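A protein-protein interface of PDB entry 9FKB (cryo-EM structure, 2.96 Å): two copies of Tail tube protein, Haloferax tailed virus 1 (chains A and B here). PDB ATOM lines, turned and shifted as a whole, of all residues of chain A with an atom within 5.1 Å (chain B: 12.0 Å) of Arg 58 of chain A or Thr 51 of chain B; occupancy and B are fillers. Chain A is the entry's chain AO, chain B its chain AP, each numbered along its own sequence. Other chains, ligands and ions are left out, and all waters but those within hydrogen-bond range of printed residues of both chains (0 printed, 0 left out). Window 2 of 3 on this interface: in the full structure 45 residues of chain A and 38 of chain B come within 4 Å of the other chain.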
ATOM      1  N   TYR A  40      27.690  -5.355   1.924  1.00  0.00           N
ATOM      2  CA  TYR A  40      27.519  -5.215   3.356  1.00  0.00           C
ATOM      3  C   TYR A  40      28.147  -6.432   4.026  1.00  0.00           C
ATOM      4  O   TYR A  40      28.308  -7.476   3.407  1.00  0.00           O
ATOM      5  CB  TYR A  40      26.034  -5.251   3.671  1.00  0.00           C
ATOM      6  CG  TYR A  40      25.172  -4.124   3.160  1.00  0.00           C
ATOM      7  CD1 TYR A  40      24.706  -4.099   1.859  1.00  0.00           C
ATOM      8  CD2 TYR A  40      24.728  -3.129   4.019  1.00  0.00           C
ATOM      9  CE1 TYR A  40      23.826  -3.116   1.432  1.00  0.00           C
ATOM     10  CE2 TYR A  40      23.822  -2.157   3.611  1.00  0.00           C
ATOM     11  CZ  TYR A  40      23.362  -2.153   2.310  1.00  0.00           C
ATOM     12  OH  TYR A  40      22.455  -1.215   1.896  1.00  0.00           O
ATOM     13  N   GLU A  41      28.491  -6.303   5.305  1.00  0.00           N
ATOM     14  CA  GLU A  41      28.748  -7.477   6.124  1.00  0.00           C
ATOM     15  C   GLU A  41      27.433  -8.121   6.547  1.00  0.00           C
ATOM     16  O   GLU A  41      26.485  -7.420   6.863  1.00  0.00           O
ATOM     17  CB  GLU A  41      29.614  -7.109   7.325  1.00  0.00           C
ATOM     18  CG  GLU A  41      31.078  -6.904   6.973  1.00  0.00           C
ATOM     19  CD  GLU A  41      31.797  -8.062   6.291  1.00  0.00           C
ATOM     20  OE1 GLU A  41      31.308  -9.215   6.370  1.00  0.00           O
ATOM     21  OE2 GLU A  41      32.868  -7.810   5.688  1.00  0.00           O
ATOM     22  N   HIS A  42      27.383  -9.458   6.546  1.00  0.00           N
ATOM     23  CA  HIS A  42      26.205 -10.190   6.977  1.00  0.00           C
ATOM     24  C   HIS A  42      26.500 -10.948   8.264  1.00  0.00           C
ATOM     25  O   HIS A  42      27.482 -11.681   8.347  1.00  0.00           O
ATOM     26  CB  HIS A  42      25.768 -11.225   5.929  1.00  0.00           C
ATOM     27  CG  HIS A  42      24.996 -10.662   4.784  1.00  0.00           C
ATOM     28  ND1 HIS A  42      24.441 -11.431   3.775  1.00  0.00           N
ATOM     29  CD2 HIS A  42      24.716  -9.370   4.518  1.00  0.00           C
ATOM     30  CE1 HIS A  42      23.819 -10.621   2.939  1.00  0.00           C
ATOM     31  NE2 HIS A  42      23.958  -9.345   3.381  1.00  0.00           N
ATOM     32  N   VAL A  56      18.997 -13.273   9.584  1.00  0.00           N
ATOM     33  CA  VAL A  56      20.170 -12.686   8.952  1.00  0.00           C
ATOM     34  C   VAL A  56      19.964 -11.181   8.830  1.00  0.00           C
ATOM     35  O   VAL A  56      18.842 -10.724   8.621  1.00  0.00           O
ATOM     36  CB  VAL A  56      20.516 -13.342   7.603  1.00  0.00           C
ATOM     37  CG1 VAL A  56      19.361 -13.300   6.607  1.00  0.00           C
ATOM     38  CG2 VAL A  56      21.776 -12.754   7.001  1.00  0.00           C
ATOM     39  N   LYS A  57      21.057 -10.427   8.974  1.00  0.00           N
ATOM     40  CA  LYS A  57      21.034  -8.971   9.025  1.00  0.00           C
ATOM     41  C   LYS A  57      22.290  -8.420   8.349  1.00  0.00           C
ATOM     42  O   LYS A  57      23.319  -9.099   8.341  1.00  0.00           O
ATOM     43  CB  LYS A  57      21.029  -8.521  10.490  1.00  0.00           C
ATOM     44  CG  LYS A  57      19.791  -8.881  11.297  1.00  0.00           C
ATOM     45  CD  LYS A  57      18.614  -7.969  10.918  1.00  0.00           C
ATOM     46  CE  LYS A  57      17.430  -7.965  11.860  1.00  0.00           C
ATOM     47  NZ  LYS A  57      16.625  -6.712  11.777  1.00  0.00           N
ATOM     48  N   ARG A  58      22.210  -7.170   7.850  1.00  0.00           N
ATOM     49  CA  ARG A  58      23.312  -6.520   7.148  1.00  0.00           C
ATOM     50  C   ARG A  58      23.772  -5.240   7.863  1.00  0.00           C
ATOM     51  O   ARG A  58      22.982  -4.541   8.484  1.00  0.00           O
ATOM     52  CB  ARG A  58      22.931  -6.293   5.680  1.00  0.00           C
ATOM     53  CG  ARG A  58      21.880  -5.226   5.437  1.00  0.00           C
ATOM     54  CD  ARG A  58      21.577  -5.046   3.962  1.00  0.00           C
ATOM     55  NE  ARG A  58      20.568  -4.019   3.711  1.00  0.00           N
ATOM     56  CZ  ARG A  58      20.035  -3.766   2.519  1.00  0.00           C
ATOM     57  NH1 ARG A  58      19.114  -2.823   2.389  1.00  0.00           N
ATOM     58  NH2 ARG A  58      20.441  -4.458   1.464  1.00  0.00           N
ATOM     59  N   TYR A  59      25.083  -4.946   7.769  1.00  0.00           N
ATOM     60  CA  TYR A  59      25.719  -3.783   8.370  1.00  0.00           C
ATOM     61  C   TYR A  59      27.022  -3.472   7.624  1.00  0.00           C
ATOM     62  O   TYR A  59      27.379  -4.209   6.713  1.00  0.00           O
ATOM     63  CB  TYR A  59      25.872  -4.031   9.871  1.00  0.00           C
ATOM     64  CG  TYR A  59      26.952  -5.018  10.244  1.00  0.00           C
ATOM     65  CD1 TYR A  59      26.796  -6.371   9.988  1.00  0.00           C
ATOM     66  CD2 TYR A  59      28.139  -4.620  10.842  1.00  0.00           C
ATOM     67  CE1 TYR A  59      27.784  -7.296  10.291  1.00  0.00           C
ATOM     68  CE2 TYR A  59      29.144  -5.534  11.136  1.00  0.00           C
ATOM     69  CZ  TYR A  59      28.984  -6.877  10.837  1.00  0.00           C
ATOM     70  OH  TYR A  59      29.991  -7.769  11.096  1.00  0.00           O
ATOM     71  N   GLU A  60      27.685  -2.348   7.944  1.00  0.00           N
ATOM     72  CA  GLU A  60      28.924  -1.914   7.283  1.00  0.00           C
ATOM     73  C   GLU A  60      28.831  -1.908   5.760  1.00  0.00           C
ATOM     74  O   GLU A  60      29.575  -2.580   5.019  1.00  0.00           O
ATOM     75  CB  GLU A  60      30.156  -2.735   7.671  1.00  0.00           C
ATOM     76  CG  GLU A  60      30.620  -2.447   9.065  1.00  0.00           C
ATOM     77  CD  GLU A  60      32.140  -2.354   9.262  1.00  0.00           C
ATOM     78  OE1 GLU A  60      32.890  -2.738   8.328  1.00  0.00           O
ATOM     79  OE2 GLU A  60      32.575  -1.862  10.338  1.00  0.00           O
ATOM     80  N   HIS A  61      27.900  -1.094   5.279  1.00  0.00           N
ATOM     81  CA  HIS A  61      27.835  -0.858   3.860  1.00  0.00           C
ATOM     82  C   HIS A  61      29.113  -0.181   3.370  1.00  0.00           C
ATOM     83  O   HIS A  61      29.646   0.722   4.013  1.00  0.00           O
ATOM     84  CB  HIS A  61      26.632   0.029   3.607  1.00  0.00           C
ATOM     85  CG  HIS A  61      26.369   0.190   2.153  1.00  0.00           C
ATOM     86  ND1 HIS A  61      26.242  -0.857   1.268  1.00  0.00           N
ATOM     87  CD2 HIS A  61      26.285   1.319   1.429  1.00  0.00           C
ATOM     88  CE1 HIS A  61      26.057  -0.359   0.051  1.00  0.00           C
ATOM     89  NE2 HIS A  61      26.063   0.988   0.127  1.00  0.00           N
ATOM     90  N   GLU B  44      38.163   3.734   9.123  1.00  0.00           N
ATOM     91  CA  GLU B  44      36.773   4.064   8.853  1.00  0.00           C
ATOM     92  C   GLU B  44      35.944   3.935  10.128  1.00  0.00           C
ATOM     93  O   GLU B  44      36.043   2.939  10.847  1.00  0.00           O
ATOM     94  CB  GLU B  44      36.256   3.153   7.745  1.00  0.00           C
ATOM     95  CG  GLU B  44      37.024   3.327   6.460  1.00  0.00           C
ATOM     96  CD  GLU B  44      36.668   2.364   5.341  1.00  0.00           C
ATOM     97  OE1 GLU B  44      37.307   1.286   5.269  1.00  0.00           O
ATOM     98  OE2 GLU B  44      35.757   2.708   4.528  1.00  0.00           O
ATOM     99  N   LEU B  45      35.107   4.940  10.402  1.00  0.00           N
ATOM    100  CA  LEU B  45      34.249   4.911  11.576  1.00  0.00           C
ATOM    101  C   LEU B  45      32.851   4.423  11.194  1.00  0.00           C
ATOM    102  O   LEU B  45      32.164   5.057  10.374  1.00  0.00           O
ATOM    103  CB  LEU B  45      34.163   6.327  12.157  1.00  0.00           C
ATOM    104  CG  LEU B  45      33.247   6.475  13.377  1.00  0.00           C
ATOM    105  CD1 LEU B  45      33.694   5.613  14.541  1.00  0.00           C
ATOM    106  CD2 LEU B  45      33.151   7.921  13.794  1.00  0.00           C
ATOM    107  N   TYR B  46      32.411   3.349  11.860  1.00  0.00           N
ATOM    108  CA  TYR B  46      31.020   2.940  11.800  1.00  0.00           C
ATOM    109  C   TYR B  46      30.510   2.727  13.217  1.00  0.00           C
ATOM    110  O   TYR B  46      31.253   2.313  14.102  1.00  0.00           O
ATOM    111  CB  TYR B  46      30.845   1.601  11.084  1.00  0.00           C
ATOM    112  CG  TYR B  46      31.163   1.539   9.607  1.00  0.00           C
ATOM    113  CD1 TYR B  46      32.465   1.375   9.155  1.00  0.00           C
ATOM    114  CD2 TYR B  46      30.143   1.521   8.668  1.00  0.00           C
ATOM    115  CE1 TYR B  46      32.743   1.259   7.802  1.00  0.00           C
ATOM    116  CE2 TYR B  46      30.404   1.406   7.313  1.00  0.00           C
ATOM    117  CZ  TYR B  46      31.710   1.268   6.877  1.00  0.00           C
ATOM    118  OH  TYR B  46      31.997   1.159   5.540  1.00  0.00           O
ATOM    119  N   THR B  47      29.213   2.979  13.380  1.00  0.00           N
ATOM    120  CA  THR B  47      28.572   2.924  14.685  1.00  0.00           C
ATOM    121  C   THR B  47      27.137   2.426  14.535  1.00  0.00           C
ATOM    122  O   THR B  47      26.619   2.340  13.434  1.00  0.00           O
ATOM    123  CB  THR B  47      28.605   4.302  15.355  1.00  0.00           C
ATOM    124  OG1 THR B  47      27.805   5.245  14.637  1.00  0.00           O
ATOM    125  CG2 THR B  47      30.002   4.861  15.469  1.00  0.00           C
ATOM    126  N   ILE B  48      26.467   2.176  15.654  1.00  0.00           N
ATOM    127  CA  ILE B  48      25.123   1.637  15.649  1.00  0.00           C
ATOM    128  C   ILE B  48      24.119   2.599  15.004  1.00  0.00           C
ATOM    129  O   ILE B  48      23.069   2.153  14.523  1.00  0.00           O
ATOM    130  CB  ILE B  48      24.837   1.102  17.074  1.00  0.00           C
ATOM    131  CG1 ILE B  48      25.451  -0.304  17.161  1.00  0.00           C
ATOM    132  CG2 ILE B  48      23.375   1.131  17.532  1.00  0.00           C
ATOM    133  CD1 ILE B  48      25.868  -0.820  18.558  1.00  0.00           C
ATOM    134  N   ASP B  49      24.450   3.896  14.919  1.00  0.00           N
ATOM    135  CA  ASP B  49      23.575   4.907  14.317  1.00  0.00           C
ATOM    136  C   ASP B  49      23.239   4.643  12.845  1.00  0.00           C
ATOM    137  O   ASP B  49      22.125   4.950  12.398  1.00  0.00           O
ATOM    138  CB  ASP B  49      24.174   6.310  14.363  1.00  0.00           C
ATOM    139  CG  ASP B  49      24.430   6.866  15.758  1.00  0.00           C
ATOM    140  OD1 ASP B  49      23.833   6.351  16.746  1.00  0.00           O
ATOM    141  OD2 ASP B  49      25.197   7.858  15.852  1.00  0.00           O
ATOM    142  N   SER B  50      24.204   4.126  12.069  1.00  0.00           N
ATOM    143  CA  SER B  50      24.038   3.963  10.629  1.00  0.00           C
ATOM    144  C   SER B  50      24.864   2.794  10.092  1.00  0.00           C
ATOM    145  O   SER B  50      25.978   2.561  10.555  1.00  0.00           O
ATOM    146  CB  SER B  50      24.406   5.242   9.940  1.00  0.00           C
ATOM    147  OG  SER B  50      24.418   5.085   8.533  1.00  0.00           O
ATOM    148  N   THR B  51      24.359   2.133   9.048  1.00  0.00           N
ATOM    149  CA  THR B  51      25.128   1.098   8.372  1.00  0.00           C
ATOM    150  C   THR B  51      26.153   1.674   7.405  1.00  0.00           C
ATOM    151  O   THR B  51      27.059   0.937   7.002  1.00  0.00           O
ATOM    152  CB  THR B  51      24.263   0.142   7.555  1.00  0.00           C
ATOM    153  OG1 THR B  51      23.588   0.925   6.560  1.00  0.00           O
ATOM    154  CG2 THR B  51      23.316  -0.657   8.425  1.00  0.00           C
ATOM    155  N   PHE B  52      25.991   2.954   7.023  1.00  0.00           N
ATOM    156  CA  PHE B  52      26.944   3.626   6.150  1.00  0.00           C
ATOM    157  C   PHE B  52      28.136   4.153   6.940  1.00  0.00           C
ATOM    158  O   PHE B  52      28.053   4.463   8.116  1.00  0.00           O
ATOM    159  CB  PHE B  52      26.301   4.835   5.481  1.00  0.00           C
ATOM    160  CG  PHE B  52      25.150   4.562   4.542  1.00  0.00           C
ATOM    161  CD1 PHE B  52      24.823   3.262   4.148  1.00  0.00           C
ATOM    162  CD2 PHE B  52      24.352   5.615   4.108  1.00  0.00           C
ATOM    163  CE1 PHE B  52      23.758   3.039   3.278  1.00  0.00           C
ATOM    164  CE2 PHE B  52      23.276   5.388   3.263  1.00  0.00           C
ATOM    165  CZ  PHE B  52      22.983   4.101   2.851  1.00  0.00           C
ATOM    166  N   ARG B  53      29.250   4.343   6.241  1.00  0.00           N
ATOM    167  CA  ARG B  53      30.454   4.901   6.827  1.00  0.00           C
ATOM    168  C   ARG B  53      30.194   6.322   7.317  1.00  0.00           C
ATOM    169  O   ARG B  53      29.626   7.140   6.589  1.00  0.00           O
ATOM    170  CB  ARG B  53      31.528   4.880   5.751  1.00  0.00           C
ATOM    171  CG  ARG B  53      32.895   5.343   6.212  1.00  0.00           C
ATOM    172  CD  ARG B  53      33.886   5.082   5.112  1.00  0.00           C
ATOM    173  NE  ARG B  53      33.721   5.885   3.898  1.00  0.00           N
ATOM    174  CZ  ARG B  53      34.155   5.502   2.696  1.00  0.00           C
ATOM    175  NH1 ARG B  53      33.927   6.273   1.645  1.00  0.00           N
ATOM    176  NH2 ARG B  53      34.768   4.331   2.571  1.00  0.00           N
ATOM    177  N   ASP B  54      30.633   6.606   8.543  1.00  0.00           N
ATOM    178  CA  ASP B  54      30.373   7.881   9.176  1.00  0.00           C
ATOM    179  C   ASP B  54      31.524   8.853   8.947  1.00  0.00           C
ATOM    180  O   ASP B  54      31.311  10.038   8.652  1.00  0.00           O
ATOM    181  CB  ASP B  54      30.097   7.672  10.659  1.00  0.00           C
ATOM    182  CG  ASP B  54      28.979   8.579  11.180  1.00  0.00           C
ATOM    183  OD1 ASP B  54      29.064   9.830  10.979  1.00  0.00           O
ATOM    184  OD2 ASP B  54      28.007   8.034  11.787  1.00  0.00           O
ATOM    185  N   GLU B  55      32.762   8.347   9.073  1.00  0.00           N
ATOM    186  CA  GLU B  55      33.985   9.097   8.783  1.00  0.00           C
ATOM    187  C   GLU B  55      35.046   8.183   8.170  1.00  0.00           C
ATOM    188  O   GLU B  55      35.011   6.970   8.358  1.00  0.00           O
ATOM    189  CB  GLU B  55      34.570   9.693  10.070  1.00  0.00           C
ATOM    190  CG  GLU B  55      33.672  10.673  10.823  1.00  0.00           C
ATOM    191  CD  GLU B  55      33.433  12.017  10.152  1.00  0.00           C
ATOM    192  OE1 GLU B  55      33.864  12.199   8.976  1.00  0.00           O
ATOM    193  OE2 GLU B  55      32.827  12.888  10.821  1.00  0.00           O
ATOM    194  N   VAL B  56      35.995   8.801   7.449  1.00  0.00           N
ATOM    195  CA  VAL B  56      37.195   8.103   7.006  1.00  0.00           C
ATOM    196  C   VAL B  56      38.388   9.039   7.127  1.00  0.00           C
ATOM    197  O   VAL B  56      38.258  10.223   6.831  1.00  0.00           O
ATOM    198  CB  VAL B  56      37.056   7.524   5.586  1.00  0.00           C
ATOM    199  CG1 VAL B  56      36.743   8.587   4.556  1.00  0.00           C
ATOM    200  CG2 VAL B  56      38.287   6.745   5.185  1.00  0.00           C
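Among the printed residues, pairs that only touch across the chains: Glu 60 of chain A with Tyr 46 of chain B, His 61 of chain A with Phe 52 of chain B, Arg 58 of chain A with Thr 51 of chain B and Tyr 59 of chain A with Thr 51 of chain B.
Position printed for both chains: 56. Of the 7 pairs that touch across the chains among the printed residues, none has its exchanged pair printed and touching as well.
The backbone carbonyl oxygen (O) of Tyr 59 of chain A is in hydrogen-bond range of the backbone NH (N) of Glu 41 of chain A (2.8 Å). The side-chain hydroxyl (OG) of Ser 50 of chain B sits at hydrogen-bond distance from the backbone NH (N) of Phe 52 of chain B (3.0 Å).
N of Glu 60 of chain A sits close to O of Thr 51 of chain B (3.5 Å). The side-chain hydroxyl of Tyr 46 of chain B lies within hydrogen-bond range of the backbone carbonyl oxygen of His 61 of chain A (2.8 Å). N of His 61 of chain A sits at hydrogen-bond distance from O of Thr 51 of chain B, 2.8 Å away.
Hydrophobic or aromatic side chains of chain B that line the printed part of chain A: Tyr 46 and Phe 52. Hydrophobic or aromatic side chains of chain A that line the printed part of chain B: His 61. Among the printed residues, 7 pairs touch across the chains. Among the printed residues, no Asp or Glu carboxylate lies within 4 Å of a Lys or Arg side-chain nitrogen of the other chain.
Arg 58 of chain A touches just one residue of chain B: Thr 51. Thr 51 of chain B touches just these residues of chain A: Arg 58 (3.9 Å), Tyr 59 (3.9 Å), Glu 60 (3.4 Å) and His 61 (2.8 Å). No residue of chain B comes within 4 Å of Tyr 40 of chain A. No residue of chain B comes within 4 Å of His 42 of chain A. Of chain B, only Tyr 46 and Thr 51 come within 4 Å of Glu 60 of chain A. His 61 of chain A touches just these residues of chain B: Tyr 46, Thr 51 and Phe 52. Of the printed residues of chain A, Tyr 46 of chain B touches Glu 60 and His 61. Printed residues of chain A within 4 Å of Phe 52 of chain B: His 61 (3.6 Å). Thr 47 of chain B touches none of the printed residues of chain A. The nearest residue of chain B that does not touch Arg 58 of chain A is Phe 52 of chain B (7.5 Å). The nearest printed residue of chain A that does not touch Tyr 46 of chain B is Tyr 59 of chain A (5.9 Å).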
